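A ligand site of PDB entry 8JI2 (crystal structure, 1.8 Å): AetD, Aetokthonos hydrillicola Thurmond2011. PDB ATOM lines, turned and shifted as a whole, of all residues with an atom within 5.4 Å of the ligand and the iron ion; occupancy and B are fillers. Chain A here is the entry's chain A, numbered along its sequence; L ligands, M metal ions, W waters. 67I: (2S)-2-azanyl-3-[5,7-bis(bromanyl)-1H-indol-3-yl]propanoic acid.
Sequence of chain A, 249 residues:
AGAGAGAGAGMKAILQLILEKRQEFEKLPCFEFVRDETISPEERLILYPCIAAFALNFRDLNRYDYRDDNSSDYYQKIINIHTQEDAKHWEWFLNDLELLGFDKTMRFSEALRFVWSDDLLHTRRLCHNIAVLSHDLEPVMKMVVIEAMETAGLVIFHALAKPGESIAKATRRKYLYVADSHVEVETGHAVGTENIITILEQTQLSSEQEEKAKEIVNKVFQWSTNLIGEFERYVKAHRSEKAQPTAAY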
ATOM      1  N   PHE A  25     -10.532   9.767   6.624  1.00  0.00           N
ATOM      2  CA  PHE A  25      -9.421   9.113   7.386  1.00  0.00           C
ATOM      3  C   PHE A  25      -9.004   9.995   8.568  1.00  0.00           C
ATOM      4  O   PHE A  25      -8.803   9.497   9.676  1.00  0.00           O
ATOM      5  CB  PHE A  25      -8.279   8.849   6.411  1.00  0.00           C
ATOM      6  CG  PHE A  25      -7.182   8.008   6.972  1.00  0.00           C
ATOM      7  CD1 PHE A  25      -7.404   6.687   7.361  1.00  0.00           C
ATOM      8  CD2 PHE A  25      -5.899   8.511   7.105  1.00  0.00           C
ATOM      9  CE1 PHE A  25      -6.369   5.920   7.849  1.00  0.00           C
ATOM     10  CE2 PHE A  25      -4.868   7.729   7.594  1.00  0.00           C
ATOM     11  CZ  PHE A  25      -5.098   6.440   7.975  1.00  0.00           C
ATOM     12  N   ILE A  51       4.000   0.275  15.576  1.00  0.00           N
ATOM     13  CA  ILE A  51       4.537   0.654  14.249  1.00  0.00           C
ATOM     14  C   ILE A  51       5.694  -0.271  13.880  1.00  0.00           C
ATOM     15  O   ILE A  51       6.013  -0.286  12.673  1.00  0.00           O
ATOM     16  CB  ILE A  51       4.944   2.136  14.238  1.00  0.00           C
ATOM     17  CG1 ILE A  51       3.747   3.047  14.566  1.00  0.00           C
ATOM     18  CG2 ILE A  51       5.534   2.467  12.883  1.00  0.00           C
ATOM     19  CD1 ILE A  51       4.126   4.469  14.991  1.00  0.00           C
ATOM     20  N   PHE A  54       5.151  -2.453  10.943  1.00  0.00           N
ATOM     21  CA  PHE A  54       4.929  -1.722   9.681  1.00  0.00           C
ATOM     22  C   PHE A  54       6.250  -1.124   9.155  1.00  0.00           C
ATOM     23  O   PHE A  54       6.566  -1.292   7.966  1.00  0.00           O
ATOM     24  CB  PHE A  54       3.928  -0.573   9.883  1.00  0.00           C
ATOM     25  CG  PHE A  54       3.867   0.329   8.691  1.00  0.00           C
ATOM     26  CD1 PHE A  54       3.062   0.012   7.632  1.00  0.00           C
ATOM     27  CD2 PHE A  54       4.755   1.405   8.573  1.00  0.00           C
ATOM     28  CE1 PHE A  54       3.083   0.759   6.463  1.00  0.00           C
ATOM     29  CE2 PHE A  54       4.732   2.159   7.429  1.00  0.00           C
ATOM     30  CZ  PHE A  54       3.875   1.857   6.386  1.00  0.00           C
ATOM     31  N   ALA A  55       7.026  -0.464  10.002  1.00  0.00           N
ATOM     32  CA  ALA A  55       8.047   0.505   9.527  1.00  0.00           C
ATOM     33  C   ALA A  55       9.158  -0.176   8.697  1.00  0.00           C
ATOM     34  O   ALA A  55       9.608   0.432   7.676  1.00  0.00           O
ATOM     35  CB  ALA A  55       8.633   1.313  10.656  1.00  0.00           C
ATOM     36  N   PHE A  58       7.864  -1.370   5.410  1.00  0.00           N
ATOM     37  CA  PHE A  58       7.663  -0.216   4.509  1.00  0.00           C
ATOM     38  C   PHE A  58       9.001   0.118   3.856  1.00  0.00           C
ATOM     39  O   PHE A  58       9.039   0.361   2.627  1.00  0.00           O
ATOM     40  CB  PHE A  58       7.122   0.987   5.251  1.00  0.00           C
ATOM     41  CG  PHE A  58       6.902   2.162   4.367  1.00  0.00           C
ATOM     42  CD1 PHE A  58       5.837   2.235   3.492  1.00  0.00           C
ATOM     43  CD2 PHE A  58       7.798   3.209   4.424  1.00  0.00           C
ATOM     44  CE1 PHE A  58       5.647   3.363   2.702  1.00  0.00           C
ATOM     45  CE2 PHE A  58       7.608   4.337   3.633  1.00  0.00           C
ATOM     46  CZ  PHE A  58       6.567   4.380   2.740  1.00  0.00           C
ATOM     47  N   ASP A  86      12.211   7.923   1.041  1.00  0.00           N
ATOM     48  CA  ASP A  86      11.172   7.386   1.963  1.00  0.00           C
ATOM     49  C   ASP A  86      11.709   6.121   2.664  1.00  0.00           C
ATOM     50  O   ASP A  86      11.257   5.862   3.821  1.00  0.00           O
ATOM     51  CB  ASP A  86       9.838   7.193   1.237  1.00  0.00           C
ATOM     52  CG  ASP A  86       9.275   8.486   0.618  1.00  0.00           C
ATOM     53  OD1 ASP A  86       9.650   9.580   1.087  1.00  0.00           O
ATOM     54  OD2 ASP A  86       8.500   8.400  -0.381  1.00  0.00           O
ATOM     55  N   HIS A  89      13.451   6.200   6.516  1.00  0.00           N
ATOM     56  CA  HIS A  89      12.688   6.689   7.684  1.00  0.00           C
ATOM     57  C   HIS A  89      12.665   5.636   8.782  1.00  0.00           C
ATOM     58  O   HIS A  89      12.436   6.007   9.972  1.00  0.00           O
ATOM     59  CB  HIS A  89      11.295   7.183   7.267  1.00  0.00           C
ATOM     60  CG  HIS A  89      11.338   8.361   6.354  1.00  0.00           C
ATOM     61  ND1 HIS A  89      10.199   8.985   5.925  1.00  0.00           N
ATOM     62  CD2 HIS A  89      12.386   9.029   5.799  1.00  0.00           C
ATOM     63  CE1 HIS A  89      10.534   9.987   5.106  1.00  0.00           C
ATOM     64  NE2 HIS A  89      11.876  10.007   4.999  1.00  0.00           N
ATOM     65  N   TRP A  90      12.917   4.368   8.462  1.00  0.00           N
ATOM     66  CA  TRP A  90      12.895   3.294   9.486  1.00  0.00           C
ATOM     67  C   TRP A  90      13.928   3.576  10.568  1.00  0.00           C
ATOM     68  O   TRP A  90      13.745   3.221  11.692  1.00  0.00           O
ATOM     69  CB  TRP A  90      13.079   1.929   8.827  1.00  0.00           C
ATOM     70  CG  TRP A  90      14.427   1.737   8.210  1.00  0.00           C
ATOM     71  CD1 TRP A  90      14.881   2.275   7.028  1.00  0.00           C
ATOM     72  CD2 TRP A  90      15.517   1.017   8.777  1.00  0.00           C
ATOM     73  NE1 TRP A  90      16.165   1.877   6.812  1.00  0.00           N
ATOM     74  CE2 TRP A  90      16.588   1.117   7.854  1.00  0.00           C
ATOM     75  CE3 TRP A  90      15.695   0.270   9.937  1.00  0.00           C
ATOM     76  CZ2 TRP A  90      17.805   0.470   8.060  1.00  0.00           C
ATOM     77  CZ3 TRP A  90      16.910  -0.354  10.144  1.00  0.00           C
ATOM     78  CH2 TRP A  90      17.938  -0.265   9.213  1.00  0.00           C
ATOM     79  N   LEU A 126      -0.047  -4.560   5.658  1.00  0.00           N
ATOM     80  CA  LEU A 126      -0.373  -3.427   4.774  1.00  0.00           C
ATOM     81  C   LEU A 126       0.630  -3.389   3.620  1.00  0.00           C
ATOM     82  O   LEU A 126       0.218  -3.363   2.460  1.00  0.00           O
ATOM     83  CB  LEU A 126      -0.327  -2.142   5.579  1.00  0.00           C
ATOM     84  CG  LEU A 126      -0.542  -0.836   4.801  1.00  0.00           C
ATOM     85  CD1 LEU A 126      -1.775  -0.861   3.934  1.00  0.00           C
ATOM     86  CD2 LEU A 126      -0.652   0.314   5.787  1.00  0.00           C
ATOM     87  N   MET A 149      -0.956   6.114  -0.482  1.00  0.00           N
ATOM     88  CA  MET A 149      -0.253   5.614   0.722  1.00  0.00           C
ATOM     89  C   MET A 149       0.405   6.803   1.452  1.00  0.00           C
ATOM     90  O   MET A 149       0.336   6.872   2.689  1.00  0.00           O
ATOM     91  CB  MET A 149       0.779   4.582   0.284  1.00  0.00           C
ATOM     92  CG  MET A 149       1.574   4.012   1.385  1.00  0.00           C
ATOM     93  SD  MET A 149       0.415   3.152   2.491  1.00  0.00           S
ATOM     94  CE  MET A 149       1.622   2.355   3.554  1.00  0.00           C
ATOM     95  N   GLU A 150       1.015   7.715   0.714  1.00  0.00           N
ATOM     96  CA  GLU A 150       1.743   8.874   1.307  1.00  0.00           C
ATOM     97  C   GLU A 150       0.719   9.848   1.898  1.00  0.00           C
ATOM     98  O   GLU A 150       1.026  10.437   2.950  1.00  0.00           O
ATOM     99  CB  GLU A 150       2.662   9.529   0.279  1.00  0.00           C
ATOM    100  CG  GLU A 150       3.810   8.641  -0.129  1.00  0.00           C
ATOM    101  CD  GLU A 150       4.828   8.398   0.986  1.00  0.00           C
ATOM    102  OE1 GLU A 150       5.442   9.360   1.409  1.00  0.00           O
ATOM    103  OE2 GLU A 150       4.927   7.278   1.480  1.00  0.00           O
ATOM    104  N   ALA A 152      -2.261   9.029   3.251  1.00  0.00           N
ATOM    105  CA  ALA A 152      -2.621   8.405   4.548  1.00  0.00           C
ATOM    106  C   ALA A 152      -1.479   8.584   5.563  1.00  0.00           C
ATOM    107  O   ALA A 152      -1.746   8.950   6.732  1.00  0.00           O
ATOM    108  CB  ALA A 152      -2.962   6.949   4.352  1.00  0.00           C
ATOM    109  N   GLY A 153      -0.259   8.289   5.159  1.00  0.00           N
ATOM    110  CA  GLY A 153       0.923   8.424   6.025  1.00  0.00           C
ATOM    111  C   GLY A 153       1.079   9.846   6.580  1.00  0.00           C
ATOM    112  O   GLY A 153       1.320  10.029   7.798  1.00  0.00           O
ATOM    113  N   ILE A 156      -1.305  10.467   9.421  1.00  0.00           N
ATOM    114  CA  ILE A 156      -0.868   9.813  10.671  1.00  0.00           C
ATOM    115  C   ILE A 156       0.224  10.656  11.332  1.00  0.00           C
ATOM    116  O   ILE A 156       0.115  10.926  12.534  1.00  0.00           O
ATOM    117  CB  ILE A 156      -0.409   8.388  10.356  1.00  0.00           C
ATOM    118  CG1 ILE A 156      -1.612   7.553   9.897  1.00  0.00           C
ATOM    119  CG2 ILE A 156       0.323   7.804  11.539  1.00  0.00           C
ATOM    120  CD1 ILE A 156      -1.199   6.199   9.315  1.00  0.00           C
ATOM    121  N   PHE A 157       1.208  11.057  10.570  1.00  0.00           N
ATOM    122  CA  PHE A 157       2.411  11.708  11.160  1.00  0.00           C
ATOM    123  C   PHE A 157       2.138  13.168  11.493  1.00  0.00           C
ATOM    124  O   PHE A 157       2.739  13.650  12.452  1.00  0.00           O
ATOM    125  CB  PHE A 157       3.649  11.401  10.312  1.00  0.00           C
ATOM    126  CG  PHE A 157       4.117  10.002  10.560  1.00  0.00           C
ATOM    127  CD1 PHE A 157       4.912   9.683  11.657  1.00  0.00           C
ATOM    128  CD2 PHE A 157       3.713   8.975   9.714  1.00  0.00           C
ATOM    129  CE1 PHE A 157       5.274   8.367  11.908  1.00  0.00           C
ATOM    130  CE2 PHE A 157       4.079   7.658   9.975  1.00  0.00           C
ATOM    131  CZ  PHE A 157       4.851   7.352  11.058  1.00  0.00           C
ATOM    132  N   TYR A 177      11.061  10.817  14.028  1.00  0.00           N
ATOM    133  CA  TYR A 177       9.989  10.019  13.363  1.00  0.00           C
ATOM    134  C   TYR A 177       8.627  10.604  13.713  1.00  0.00           C
ATOM    135  O   TYR A 177       7.886  10.927  12.808  1.00  0.00           O
ATOM    136  CB  TYR A 177      10.129   8.549  13.772  1.00  0.00           C
ATOM    137  CG  TYR A 177       9.283   7.595  12.970  1.00  0.00           C
ATOM    138  CD1 TYR A 177       9.567   7.333  11.651  1.00  0.00           C
ATOM    139  CD2 TYR A 177       8.217   6.904  13.540  1.00  0.00           C
ATOM    140  CE1 TYR A 177       8.838   6.421  10.888  1.00  0.00           C
ATOM    141  CE2 TYR A 177       7.485   5.972  12.808  1.00  0.00           C
ATOM    142  CZ  TYR A 177       7.789   5.733  11.484  1.00  0.00           C
ATOM    143  OH  TYR A 177       7.088   4.821  10.733  1.00  0.00           O
ATOM    144  N   HIS A 182       9.868  14.973   9.986  1.00  0.00           N
ATOM    145  CA  HIS A 182       9.367  13.821   9.177  1.00  0.00           C
ATOM    146  C   HIS A 182       8.241  14.285   8.238  1.00  0.00           C
ATOM    147  O   HIS A 182       8.290  13.950   7.031  1.00  0.00           O
ATOM    148  CB  HIS A 182       8.916  12.692  10.122  1.00  0.00           C
ATOM    149  CG  HIS A 182       8.574  11.419   9.419  1.00  0.00           C
ATOM    150  ND1 HIS A 182       8.067  10.358  10.142  1.00  0.00           N
ATOM    151  CD2 HIS A 182       8.618  11.029   8.129  1.00  0.00           C
ATOM    152  CE1 HIS A 182       7.829   9.365   9.320  1.00  0.00           C
ATOM    153  NE2 HIS A 182       8.147   9.723   8.060  1.00  0.00           N
ATOM    154  N   GLU A 186       8.805  14.485   4.105  1.00  0.00           N
ATOM    155  CA  GLU A 186       7.881  13.526   3.431  1.00  0.00           C
ATOM    156  C   GLU A 186       7.046  14.250   2.367  1.00  0.00           C
ATOM    157  O   GLU A 186       6.976  13.749   1.245  1.00  0.00           O
ATOM    158  CB  GLU A 186       6.952  12.827   4.419  1.00  0.00           C
ATOM    159  CG  GLU A 186       6.302  11.574   3.873  1.00  0.00           C
ATOM    160  CD  GLU A 186       6.952  10.255   4.256  1.00  0.00           C
ATOM    161  OE1 GLU A 186       7.600  10.239   5.270  1.00  0.00           O
ATOM    162  OE2 GLU A 186       6.749   9.222   3.558  1.00  0.00           O
ATOM    163  N   SER A 224      -5.274   1.080   5.290  1.00  0.00           N
ATOM    164  CA  SER A 224      -4.786   2.083   6.255  1.00  0.00           C
ATOM    165  C   SER A 224      -5.776   2.232   7.411  1.00  0.00           C
ATOM    166  O   SER A 224      -5.363   2.318   8.584  1.00  0.00           O
ATOM    167  CB  SER A 224      -4.583   3.399   5.590  1.00  0.00           C
ATOM    168  OG  SER A 224      -3.551   3.293   4.622  1.00  0.00           O
ATOM    169  N   LEU A 227      -5.367  -0.732   9.717  1.00  0.00           N
ATOM    170  CA  LEU A 227      -4.158  -0.532  10.554  1.00  0.00           C
ATOM    171  C   LEU A 227      -4.535   0.391  11.731  1.00  0.00           C
ATOM    172  O   LEU A 227      -4.248   0.071  12.911  1.00  0.00           O
ATOM    173  CB  LEU A 227      -3.018  -0.002   9.643  1.00  0.00           C
ATOM    174  CG  LEU A 227      -1.722   0.415  10.345  1.00  0.00           C
ATOM    175  CD1 LEU A 227      -0.575   0.434   9.324  1.00  0.00           C
ATOM    176  CD2 LEU A 227      -1.841   1.791  11.005  1.00  0.00           C
ATOM    177  N   PHE A 231      -4.378   0.081  15.975  1.00  0.00           N
ATOM    178  CA  PHE A 231      -3.726   1.013  16.919  1.00  0.00           C
ATOM    179  C   PHE A 231      -4.758   1.384  17.989  1.00  0.00           C
ATOM    180  O   PHE A 231      -4.416   1.410  19.172  1.00  0.00           O
ATOM    181  CB  PHE A 231      -3.152   2.226  16.232  1.00  0.00           C
ATOM    182  CG  PHE A 231      -1.938   1.977  15.371  1.00  0.00           C
ATOM    183  CD1 PHE A 231      -1.480   0.711  15.113  1.00  0.00           C
ATOM    184  CD2 PHE A 231      -1.258   3.049  14.815  1.00  0.00           C
ATOM    185  CE1 PHE A 231      -0.392   0.486  14.271  1.00  0.00           C
ATOM    186  CE2 PHE A 231      -0.164   2.837  13.982  1.00  0.00           C
ATOM    187  CZ  PHE A 231       0.289   1.567  13.735  1.00  0.00           C
HETATM  188  OXT 67I L   1       7.460   4.936   8.090  1.00  0.00           O
HETATM  189  C   67I L   1       7.417   6.095   7.538  1.00  0.00           C
HETATM  190  O   67I L   1       8.472   6.778   7.358  1.00  0.00           O
HETATM  191  CA  67I L   1       6.015   6.612   7.092  1.00  0.00           C
HETATM  192  N   67I L   1       6.067   8.012   6.601  1.00  0.00           N
HETATM  193  CB  67I L   1       5.410   5.762   6.020  1.00  0.00           C
HETATM  194  CG  67I L   1       3.857   5.581   5.864  1.00  0.00           C
HETATM  195  CD2 67I L   1       3.024   5.074   6.818  1.00  0.00           C
HETATM  196  CE3 67I L   1       3.093   4.633   8.113  1.00  0.00           C
HETATM  197  CZ3 67I L   1       1.995   4.042   8.853  1.00  0.00           C
HETATM  198 BR1  67I L   1       2.212   3.564  10.583  1.00  0.00          BR
HETATM  199  CH2 67I L   1       0.826   3.964   8.142  1.00  0.00           C
HETATM  200  CZ2 67I L   1       0.827   4.401   6.877  1.00  0.00           C
HETATM  201 BR2  67I L   1      -0.920   4.186   5.869  1.00  0.00          BR
HETATM  202  CE2 67I L   1       1.823   4.952   6.199  1.00  0.00           C
HETATM  203  NE1 67I L   1       1.934   5.350   4.952  1.00  0.00           N
HETATM  204  CD1 67I L   1       3.177   5.774   4.718  1.00  0.00           C
HETATM  205 FE    FE M   1       8.168   8.518   6.379  1.00  0.00          FE
HETATM  206  O   HOH W   1       9.776   3.327   7.660  1.00  0.00           O
HETATM  207  O   HOH W   2       8.210   7.453   4.673  1.00  0.00           O
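ND1 of His 182 sits at hydrogen-bond distance from O of Tyr 177, at 2.7 Å. The side-chain carboxylate (OE2) of Glu 186 lies close to the side-chain carboxylate (OE1) of Glu 150 (2.5 Å).
Water W2 is bound to the iron ion, 2.0 Å away. O of the ligand binds the iron ion (2.0 Å). A ring nitrogen (NE2) of His 182 is bound to the iron ion. The iron ion is bound by OE1 of Glu 186. A ring nitrogen (ND1) of His 89 binds the iron ion, at 2.1 Å. N of the ligand is bound to the iron ion (2.2 Å).
Water W1 lies within hydrogen-bond range of OXT of the ligand, O of Ala 55 and N of Trp 90.
Merely in contact with the ligand: Ser 224 (3.0 Å), Phe 54 (3.0 Å), Ile 156 (3.2 Å), Gly 153 (3.4 Å), Phe 58 (3.5 Å), Phe 157 (3.6 Å), Ala 152 (3.8 Å), Leu 126 (3.9 Å), Glu 150 (3.98 Å) and Leu 227 (3.98 Å). Hydrophobic or aromatic side chains that line the ligand: Phe 54, Phe 58, His 89, Leu 126, Met 149, Ala 152, Ile 156, Phe 157, Tyr 177, His 182 and Leu 227. Within 4 Å of the ligand: Phe 54, Phe 58, His 89, Leu 126, Met 149, Glu 150, Ala 152, Gly 153, Ile 156, Phe 157, Tyr 177, His 182, Glu 186, Ser 224 and Leu 227.
OH of Tyr 177 lies within hydrogen-bond range of OXT of the ligand (2.7 Å). The backbone carbonyl oxygen of Met 149 lies within hydrogen-bond range of a nitrogen (NE1) of the ligand (3.2 Å). The side-chain sulfur (SD) of Met 149 sits close to a nitrogen (NE1) of the ligand (3.6 Å).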
